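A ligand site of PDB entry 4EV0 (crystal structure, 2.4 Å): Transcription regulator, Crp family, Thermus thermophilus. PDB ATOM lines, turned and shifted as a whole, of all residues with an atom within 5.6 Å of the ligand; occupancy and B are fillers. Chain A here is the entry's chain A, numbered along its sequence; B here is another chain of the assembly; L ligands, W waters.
The backbone NH of Gly 75 sits at hydrogen-bond distance from an oxygen (O6) of the ligand (3.0 Å).
The backbone NH (N) of Ser 78 is in hydrogen-bond range of an oxygen (O1) of the ligand (3.0 Å).
A nitrogen (N4) of the ligand sits close to the guanidinium group (NH1) of Arg 126 (3.3 Å).
The backbone NH (N) of Met 77 is in hydrogen-bond range of an oxygen (O1) of the ligand.
An oxygen (O1) of the ligand is in salt-bridge range of the guanidinium group (NH1) of Arg 85 (3.1 Å).
OE1 of Glu 76 lies within hydrogen-bond range of O6 of the ligand (2.5 Å).
An oxygen (O1) of the ligand is in hydrogen-bond range of the side-chain hydroxyl (OG) of Ser 78, at 3.3 Å.
N of Ser 86 is in hydrogen-bond range of O2 of the ligand (2.8 Å).
The side-chain hydroxyl (OG) of Ser 86 sits at hydrogen-bond distance from an oxygen (O2) of the ligand (2.9 Å).
The backbone carbonyl oxygen (O) of Ser 86 lies within hydrogen-bond range of the guanidinium group (NH1) of Arg 55 (3.0 Å).
The side-chain hydroxyl (OG) of Ser 78 lies close to the backbone NH (N) of Arg 85 (3.3 Å).
O of Gly 75 lies within hydrogen-bond range of NH1 of Arg 85.
The backbone NH of Leu 53 lies within hydrogen-bond range of the backbone carbonyl oxygen of Ala 66 (3.0 Å).
O of Glu 84 lies close to OG of Ser 78, at 3.3 Å.
N of Leu 65 is in hydrogen-bond range of O of Leu 53.
The guanidinium group of Arg 126 is in salt-bridge range of the side-chain carboxylate of Glu 76 (3.8 Å).
CZ of Phe 34 touches O3 of the ligand (3.6 Å).
CD1 of Leu 53 touches O4 of the ligand (3.6 Å).
Leu 65 touches the ligand (CD1 to N2, 3.5 Å).
CA of Phe 74 touches O6 of the ligand, at 3.4 Å.
Ala 87 touches the ligand.
Hydrophobic or aromatic side chains that line the ligand: Phe 34, Leu 53, Leu 65, Phe 74, Met 77 and Ala 87.
Of the 23 residues printed, 12 come within 4 Å of the ligand.
The nearest printed residue that does not touch the ligand is Glu 84 (4.1 Å).
Water W1 lies within hydrogen-bond range of NH1 of Arg 126 (3.0 Å) and N3 of the ligand (3.1 Å).
Water W2 lies within hydrogen-bond range of the side-chain carboxylate of Asp 131 of chain B (2.6 Å), the side-chain hydroxyl of Ser 86 (2.9 Å), the guanidinium group of Arg 126 (3.2 Å) and a nitrogen (N2) of the ligand (3.4 Å).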
ATOM      1  N   PHE A  34     -29.167 -11.995   6.954  1.00  0.00           N
ATOM      2  CA  PHE A  34     -29.149 -12.383   5.546  1.00  0.00           C
ATOM      3  C   PHE A  34     -29.841 -13.723   5.331  1.00  0.00           C
ATOM      4  O   PHE A  34     -30.060 -14.473   6.274  1.00  0.00           O
ATOM      5  CB  PHE A  34     -27.728 -12.374   4.948  1.00  0.00           C
ATOM      6  CG  PHE A  34     -26.709 -13.243   5.672  1.00  0.00           C
ATOM      7  CD1 PHE A  34     -26.863 -14.633   5.736  1.00  0.00           C
ATOM      8  CD2 PHE A  34     -25.564 -12.670   6.218  1.00  0.00           C
ATOM      9  CE1 PHE A  34     -25.909 -15.454   6.370  1.00  0.00           C
ATOM     10  CE2 PHE A  34     -24.581 -13.469   6.858  1.00  0.00           C
ATOM     11  CZ  PHE A  34     -24.770 -14.872   6.942  1.00  0.00           C
ATOM     12  N   LEU A  53     -28.119 -19.291  13.017  1.00  0.00           N
ATOM     13  CA  LEU A  53     -27.823 -19.678  11.649  1.00  0.00           C
ATOM     14  C   LEU A  53     -28.630 -20.900  11.325  1.00  0.00           C
ATOM     15  O   LEU A  53     -28.668 -21.849  12.099  1.00  0.00           O
ATOM     16  CB  LEU A  53     -26.354 -20.023  11.472  1.00  0.00           C
ATOM     17  CG  LEU A  53     -25.321 -18.940  11.744  1.00  0.00           C
ATOM     18  CD1 LEU A  53     -23.929 -19.546  11.625  1.00  0.00           C
ATOM     19  CD2 LEU A  53     -25.512 -17.795  10.766  1.00  0.00           C
ATOM     20  N   ARG A  55     -30.160 -23.489   7.814  1.00  0.00           N
ATOM     21  CA  ARG A  55     -30.022 -23.847   6.420  1.00  0.00           C
ATOM     22  C   ARG A  55     -31.311 -24.539   5.946  1.00  0.00           C
ATOM     23  O   ARG A  55     -31.998 -25.198   6.725  1.00  0.00           O
ATOM     24  CB  ARG A  55     -28.768 -24.726   6.252  1.00  0.00           C
ATOM     25  CG  ARG A  55     -28.450 -25.161   4.829  1.00  0.00           C
ATOM     26  CD  ARG A  55     -26.975 -25.600   4.685  1.00  0.00           C
ATOM     27  NE  ARG A  55     -26.779 -26.453   3.517  1.00  0.00           N
ATOM     28  CZ  ARG A  55     -26.616 -26.018   2.268  1.00  0.00           C
ATOM     29  NH1 ARG A  55     -26.604 -24.727   2.004  1.00  0.00           N
ATOM     30  NH2 ARG A  55     -26.442 -26.897   1.264  1.00  0.00           N
ATOM     31  N   ARG A  63     -32.857 -26.706   9.052  1.00  0.00           N
ATOM     32  CA  ARG A  63     -31.964 -27.240  10.070  1.00  0.00           C
ATOM     33  C   ARG A  63     -31.178 -26.088  10.718  1.00  0.00           C
ATOM     34  O   ARG A  63     -30.581 -25.265  10.018  1.00  0.00           O
ATOM     35  CB  ARG A  63     -30.983 -28.252   9.443  1.00  0.00           C
ATOM     36  CG  ARG A  63     -30.093 -28.992  10.448  1.00  0.00           C
ATOM     37  CD  ARG A  63     -28.735 -29.419   9.857  1.00  0.00           C
ATOM     38  NE  ARG A  63     -27.894 -30.079  10.847  1.00  0.00           N
ATOM     39  CZ  ARG A  63     -26.593 -30.353  10.686  1.00  0.00           C
ATOM     40  NH1 ARG A  63     -25.965 -30.006   9.569  1.00  0.00           N
ATOM     41  NH2 ARG A  63     -25.921 -30.964  11.648  1.00  0.00           N
ATOM     42  N   LEU A  65     -28.076 -24.532  12.451  1.00  0.00           N
ATOM     43  CA  LEU A  65     -26.653 -24.869  12.406  1.00  0.00           C
ATOM     44  C   LEU A  65     -25.944 -24.515  13.692  1.00  0.00           C
ATOM     45  O   LEU A  65     -25.082 -25.259  14.167  1.00  0.00           O
ATOM     46  CB  LEU A  65     -25.964 -24.150  11.249  1.00  0.00           C
ATOM     47  CG  LEU A  65     -26.505 -24.522   9.882  1.00  0.00           C
ATOM     48  CD1 LEU A  65     -25.678 -23.849   8.808  1.00  0.00           C
ATOM     49  CD2 LEU A  65     -26.535 -26.041   9.688  1.00  0.00           C
ATOM     50  N   ALA A  66     -26.310 -23.357  14.234  1.00  0.00           N
ATOM     51  CA  ALA A  66     -25.692 -22.858  15.451  1.00  0.00           C
ATOM     52  C   ALA A  66     -26.461 -21.681  16.019  1.00  0.00           C
ATOM     53  O   ALA A  66     -27.301 -21.072  15.344  1.00  0.00           O
ATOM     54  CB  ALA A  66     -24.245 -22.467  15.200  1.00  0.00           C
ATOM     55  N   LEU A  73     -17.832 -15.645  14.982  1.00  0.00           N
ATOM     56  CA  LEU A  73     -17.762 -15.227  13.582  1.00  0.00           C
ATOM     57  C   LEU A  73     -18.669 -16.057  12.632  1.00  0.00           C
ATOM     58  O   LEU A  73     -18.867 -17.254  12.841  1.00  0.00           O
ATOM     59  CB  LEU A  73     -16.306 -15.342  13.133  1.00  0.00           C
ATOM     60  CG  LEU A  73     -16.104 -15.324  11.623  1.00  0.00           C
ATOM     61  CD1 LEU A  73     -15.746 -13.910  11.144  1.00  0.00           C
ATOM     62  CD2 LEU A  73     -15.073 -16.356  11.211  1.00  0.00           C
ATOM     63  N   PHE A  74     -19.194 -15.403  11.594  1.00  0.00           N
ATOM     64  CA  PHE A  74     -19.966 -16.087  10.561  1.00  0.00           C
ATOM     65  C   PHE A  74     -19.986 -15.272   9.266  1.00  0.00           C
ATOM     66  O   PHE A  74     -19.582 -14.101   9.252  1.00  0.00           O
ATOM     67  CB  PHE A  74     -21.405 -16.379  11.023  1.00  0.00           C
ATOM     68  CG  PHE A  74     -22.250 -15.134  11.294  1.00  0.00           C
ATOM     69  CD1 PHE A  74     -22.219 -14.508  12.524  1.00  0.00           C
ATOM     70  CD2 PHE A  74     -23.100 -14.625  10.316  1.00  0.00           C
ATOM     71  CE1 PHE A  74     -23.016 -13.383  12.777  1.00  0.00           C
ATOM     72  CE2 PHE A  74     -23.894 -13.491  10.551  1.00  0.00           C
ATOM     73  CZ  PHE A  74     -23.854 -12.879  11.788  1.00  0.00           C
ATOM     74  N   GLY A  75     -20.476 -15.893   8.192  1.00  0.00           N
ATOM     75  CA  GLY A  75     -20.525 -15.230   6.905  1.00  0.00           C
ATOM     76  C   GLY A  75     -19.182 -15.179   6.179  1.00  0.00           C
ATOM     77  O   GLY A  75     -19.000 -14.389   5.260  1.00  0.00           O
ATOM     78  N   GLU A  76     -18.232 -16.020   6.575  1.00  0.00           N
ATOM     79  CA  GLU A  76     -16.908 -16.009   5.949  1.00  0.00           C
ATOM     80  C   GLU A  76     -16.880 -16.585   4.516  1.00  0.00           C
ATOM     81  O   GLU A  76     -16.047 -16.183   3.703  1.00  0.00           O
ATOM     82  CB  GLU A  76     -15.875 -16.702   6.845  1.00  0.00           C
ATOM     83  CG  GLU A  76     -16.009 -18.221   6.926  1.00  0.00           C
ATOM     84  CD  GLU A  76     -17.225 -18.694   7.724  1.00  0.00           C
ATOM     85  OE1 GLU A  76     -17.823 -17.875   8.449  1.00  0.00           O
ATOM     86  OE2 GLU A  76     -17.558 -19.909   7.638  1.00  0.00           O
ATOM     87  N   MET A  77     -17.788 -17.514   4.208  1.00  0.00           N
ATOM     88  CA  MET A  77     -17.820 -18.135   2.877  1.00  0.00           C
ATOM     89  C   MET A  77     -17.961 -17.152   1.713  1.00  0.00           C
ATOM     90  O   MET A  77     -17.080 -17.098   0.846  1.00  0.00           O
ATOM     91  CB  MET A  77     -18.956 -19.149   2.757  1.00  0.00           C
ATOM     92  CG  MET A  77     -18.962 -20.234   3.797  1.00  0.00           C
ATOM     93  SD  MET A  77     -17.693 -21.488   3.600  1.00  0.00           S
ATOM     94  CE  MET A  77     -17.778 -22.147   5.262  1.00  0.00           C
ATOM     95  N   SER A  78     -19.071 -16.415   1.678  1.00  0.00           N
ATOM     96  CA  SER A  78     -19.304 -15.438   0.619  1.00  0.00           C
ATOM     97  C   SER A  78     -18.201 -14.390   0.591  1.00  0.00           C
ATOM     98  O   SER A  78     -17.844 -13.870  -0.466  1.00  0.00           O
ATOM     99  CB  SER A  78     -20.640 -14.709   0.799  1.00  0.00           C
ATOM    100  OG  SER A  78     -21.704 -15.630   0.875  1.00  0.00           O
ATOM    101  N   LEU A  79     -17.675 -14.077   1.777  1.00  0.00           N
ATOM    102  CA  LEU A  79     -16.577 -13.141   1.840  1.00  0.00           C
ATOM    103  C   LEU A  79     -15.416 -13.703   1.019  1.00  0.00           C
ATOM    104  O   LEU A  79     -14.838 -13.011   0.170  1.00  0.00           O
ATOM    105  CB  LEU A  79     -16.109 -12.913   3.280  1.00  0.00           C
ATOM    106  CG  LEU A  79     -14.895 -11.993   3.219  1.00  0.00           C
ATOM    107  CD1 LEU A  79     -15.270 -10.576   3.571  1.00  0.00           C
ATOM    108  CD2 LEU A  79     -13.745 -12.505   4.068  1.00  0.00           C
ATOM    109  N   GLU A  84     -22.879 -17.846  -2.881  1.00  0.00           N
ATOM    110  CA  GLU A  84     -24.063 -17.598  -2.065  1.00  0.00           C
ATOM    111  C   GLU A  84     -23.776 -17.812  -0.587  1.00  0.00           C
ATOM    112  O   GLU A  84     -22.880 -18.560  -0.233  1.00  0.00           O
ATOM    113  CB  GLU A  84     -25.192 -18.546  -2.434  1.00  0.00           C
ATOM    114  CG  GLU A  84     -24.938 -20.019  -2.054  1.00  0.00           C
ATOM    115  CD  GLU A  84     -26.137 -20.940  -2.332  1.00  0.00           C
ATOM    116  OE1 GLU A  84     -27.053 -20.512  -3.067  1.00  0.00           O
ATOM    117  OE2 GLU A  84     -26.160 -22.083  -1.824  1.00  0.00           O
ATOM    118  N   ARG A  85     -24.558 -17.166   0.267  1.00  0.00           N
ATOM    119  CA  ARG A  85     -24.611 -17.543   1.678  1.00  0.00           C
ATOM    120  C   ARG A  85     -25.132 -18.976   1.743  1.00  0.00           C
ATOM    121  O   ARG A  85     -26.173 -19.297   1.162  1.00  0.00           O
ATOM    122  CB  ARG A  85     -25.585 -16.642   2.444  1.00  0.00           C
ATOM    123  CG  ARG A  85     -25.260 -15.159   2.436  1.00  0.00           C
ATOM    124  CD  ARG A  85     -23.950 -14.899   3.161  1.00  0.00           C
ATOM    125  NE  ARG A  85     -23.745 -13.467   3.412  1.00  0.00           N
ATOM    126  CZ  ARG A  85     -22.620 -12.948   3.904  1.00  0.00           C
ATOM    127  NH1 ARG A  85     -21.586 -13.743   4.180  1.00  0.00           N
ATOM    128  NH2 ARG A  85     -22.525 -11.625   4.103  1.00  0.00           N
ATOM    129  N   SER A  86     -24.430 -19.829   2.474  1.00  0.00           N
ATOM    130  CA  SER A  86     -24.851 -21.234   2.549  1.00  0.00           C
ATOM    131  C   SER A  86     -25.792 -21.461   3.738  1.00  0.00           C
ATOM    132  O   SER A  86     -26.169 -22.595   4.026  1.00  0.00           O
ATOM    133  CB  SER A  86     -23.641 -22.156   2.668  1.00  0.00           C
ATOM    134  OG  SER A  86     -22.936 -21.923   3.881  1.00  0.00           O
ATOM    135  N   ALA A  87     -26.135 -20.386   4.434  1.00  0.00           N
ATOM    136  CA  ALA A  87     -27.128 -20.455   5.512  1.00  0.00           C
ATOM    137  C   ALA A  87     -27.807 -19.108   5.705  1.00  0.00           C
ATOM    138  O   ALA A  87     -27.320 -18.085   5.233  1.00  0.00           O
ATOM    139  CB  ALA A  87     -26.478 -20.903   6.824  1.00  0.00           C
ATOM    140  N   SER A  88     -28.933 -19.110   6.406  1.00  0.00           N
ATOM    141  CA  SER A  88     -29.567 -17.851   6.745  1.00  0.00           C
ATOM    142  C   SER A  88     -29.127 -17.453   8.151  1.00  0.00           C
ATOM    143  O   SER A  88     -28.776 -18.331   8.964  1.00  0.00           O
ATOM    144  CB  SER A  88     -31.100 -17.964   6.678  1.00  0.00           C
ATOM    145  OG  SER A  88     -31.549 -18.093   5.337  1.00  0.00           O
ATOM    146  N   ARG A 126     -13.620 -26.461  10.555  1.00  0.00           N
ATOM    147  CA  ARG A 126     -14.958 -26.805  10.089  1.00  0.00           C
ATOM    148  C   ARG A 126     -14.925 -27.982   9.114  1.00  0.00           C
ATOM    149  O   ARG A 126     -15.806 -28.841   9.130  1.00  0.00           O
ATOM    150  CB  ARG A 126     -15.676 -25.576   9.501  1.00  0.00           C
ATOM    151  CG  ARG A 126     -16.657 -24.928  10.488  1.00  0.00           C
ATOM    152  CD  ARG A 126     -17.304 -23.603   9.995  1.00  0.00           C
ATOM    153  NE  ARG A 126     -17.921 -23.588   8.663  1.00  0.00           N
ATOM    154  CZ  ARG A 126     -18.656 -24.564   8.102  1.00  0.00           C
ATOM    155  NH1 ARG A 126     -18.909 -25.711   8.747  1.00  0.00           N
ATOM    156  NH2 ARG A 126     -19.156 -24.389   6.883  1.00  0.00           N
ATOM    157  N   GLU A 129     -14.761 -31.184  10.987  1.00  0.00           N
ATOM    158  CA  GLU A 129     -16.093 -31.536  11.484  1.00  0.00           C
ATOM    159  C   GLU A 129     -16.933 -32.146  10.374  1.00  0.00           C
ATOM    160  O   GLU A 129     -17.711 -33.073  10.602  1.00  0.00           O
ATOM    161  CB  GLU A 129     -16.797 -30.308  12.079  1.00  0.00           C
ATOM    162  CG  GLU A 129     -16.502 -30.033  13.566  1.00  0.00           C
ATOM    163  CD  GLU A 129     -16.804 -28.583  14.006  1.00  0.00           C
ATOM    164  OE1 GLU A 129     -17.334 -27.790  13.186  1.00  0.00           O
ATOM    165  OE2 GLU A 129     -16.509 -28.231  15.170  1.00  0.00           O
ATOM    166  N   GLU A 133     -18.741 -35.829   9.768  1.00  0.00           N
ATOM    167  CA  GLU A 133     -20.150 -35.954   9.433  1.00  0.00           C
ATOM    168  C   GLU A 133     -20.357 -36.793   8.187  1.00  0.00           C
ATOM    169  O   GLU A 133     -21.304 -37.561   8.113  1.00  0.00           O
ATOM    170  CB  GLU A 133     -20.816 -34.587   9.242  1.00  0.00           C
ATOM    171  CG  GLU A 133     -21.031 -33.824  10.520  1.00  0.00           C
ATOM    172  CD  GLU A 133     -21.838 -32.540  10.329  1.00  0.00           C
ATOM    173  OE1 GLU A 133     -23.040 -32.666   9.976  1.00  0.00           O
ATOM    174  OE2 GLU A 133     -21.283 -31.418  10.544  1.00  0.00           O
ATOM    175  N   ARG B 128     -17.930 -26.249   0.341  1.00  0.00           N
ATOM    176  CA  ARG B 128     -19.073 -26.167  -0.543  1.00  0.00           C
ATOM    177  C   ARG B 128     -19.359 -27.501  -1.226  1.00  0.00           C
ATOM    178  O   ARG B 128     -20.509 -27.924  -1.344  1.00  0.00           O
ATOM    179  CB  ARG B 128     -18.889 -25.046  -1.566  1.00  0.00           C
ATOM    180  CG  ARG B 128     -19.111 -23.674  -0.947  1.00  0.00           C
ATOM    181  CD  ARG B 128     -19.236 -22.586  -1.998  1.00  0.00           C
ATOM    182  NE  ARG B 128     -19.125 -21.248  -1.414  1.00  0.00           N
ATOM    183  CZ  ARG B 128     -20.159 -20.556  -0.947  1.00  0.00           C
ATOM    184  NH1 ARG B 128     -21.384 -21.074  -0.980  1.00  0.00           N
ATOM    185  NH2 ARG B 128     -19.970 -19.341  -0.434  1.00  0.00           N
ATOM    186  N   ASP B 131     -21.037 -29.663   1.403  1.00  0.00           N
ATOM    187  CA  ASP B 131     -22.469 -29.406   1.611  1.00  0.00           C
ATOM    188  C   ASP B 131     -23.271 -30.114   0.526  1.00  0.00           C
ATOM    189  O   ASP B 131     -24.368 -30.632   0.778  1.00  0.00           O
ATOM    190  CB  ASP B 131     -22.788 -27.901   1.610  1.00  0.00           C
ATOM    191  CG  ASP B 131     -22.472 -27.215   2.946  1.00  0.00           C
ATOM    192  OD1 ASP B 131     -22.831 -27.762   4.012  1.00  0.00           O
ATOM    193  OD2 ASP B 131     -21.863 -26.111   2.936  1.00  0.00           O
HETATM  194  P1  LIG L   1     -21.721 -17.957   4.567  1.00  0.00           P
HETATM  195  O1  LIG L   1     -21.081 -16.753   3.920  1.00  0.00           O
HETATM  196  O2  LIG L   1     -21.956 -19.206   3.721  1.00  0.00           O
HETATM  197  O3  LIG L   1     -23.111 -17.535   5.275  1.00  0.00           O
HETATM  198  C1  LIG L   1     -23.704 -18.365   6.267  1.00  0.00           C
HETATM  199  C2  LIG L   1     -22.648 -18.793   7.222  1.00  0.00           C
HETATM  200  O4  LIG L   1     -23.062 -19.853   8.109  1.00  0.00           O
HETATM  201  C3  LIG L   1     -21.430 -19.380   6.581  1.00  0.00           C
HETATM  202  O5  LIG L   1     -20.747 -18.426   5.792  1.00  0.00           O
HETATM  203  C4  LIG L   1     -20.697 -19.894   7.796  1.00  0.00           C
HETATM  204  O6  LIG L   1     -20.174 -18.810   8.543  1.00  0.00           O
HETATM  205  C5  LIG L   1     -21.880 -20.487   8.596  1.00  0.00           C
HETATM  206  N1  LIG L   1     -22.014 -21.940   8.403  1.00  0.00           N
HETATM  207  C6  LIG L   1     -22.412 -22.546   7.274  1.00  0.00           C
HETATM  208  N2  LIG L   1     -22.452 -23.897   7.424  1.00  0.00           N
HETATM  209  C7  LIG L   1     -22.089 -24.172   8.679  1.00  0.00           C
HETATM  210  C8  LIG L   1     -21.940 -25.408   9.467  1.00  0.00           C
HETATM  211  N3  LIG L   1     -22.191 -26.629   8.905  1.00  0.00           N
HETATM  212  N4  LIG L   1     -21.531 -25.267  10.750  1.00  0.00           N
HETATM  213  C9  LIG L   1     -21.277 -24.059  11.294  1.00  0.00           C
HETATM  214  N5  LIG L   1     -21.407 -22.890  10.624  1.00  0.00           N
HETATM  215  C10 LIG L   1     -21.797 -22.879   9.331  1.00  0.00           C
HETATM  216  O   HOH W   1     -19.810 -28.541   9.091  1.00  0.00           O
HETATM  217  O   HOH W   2     -21.036 -24.104   4.319  1.00  0.00           O
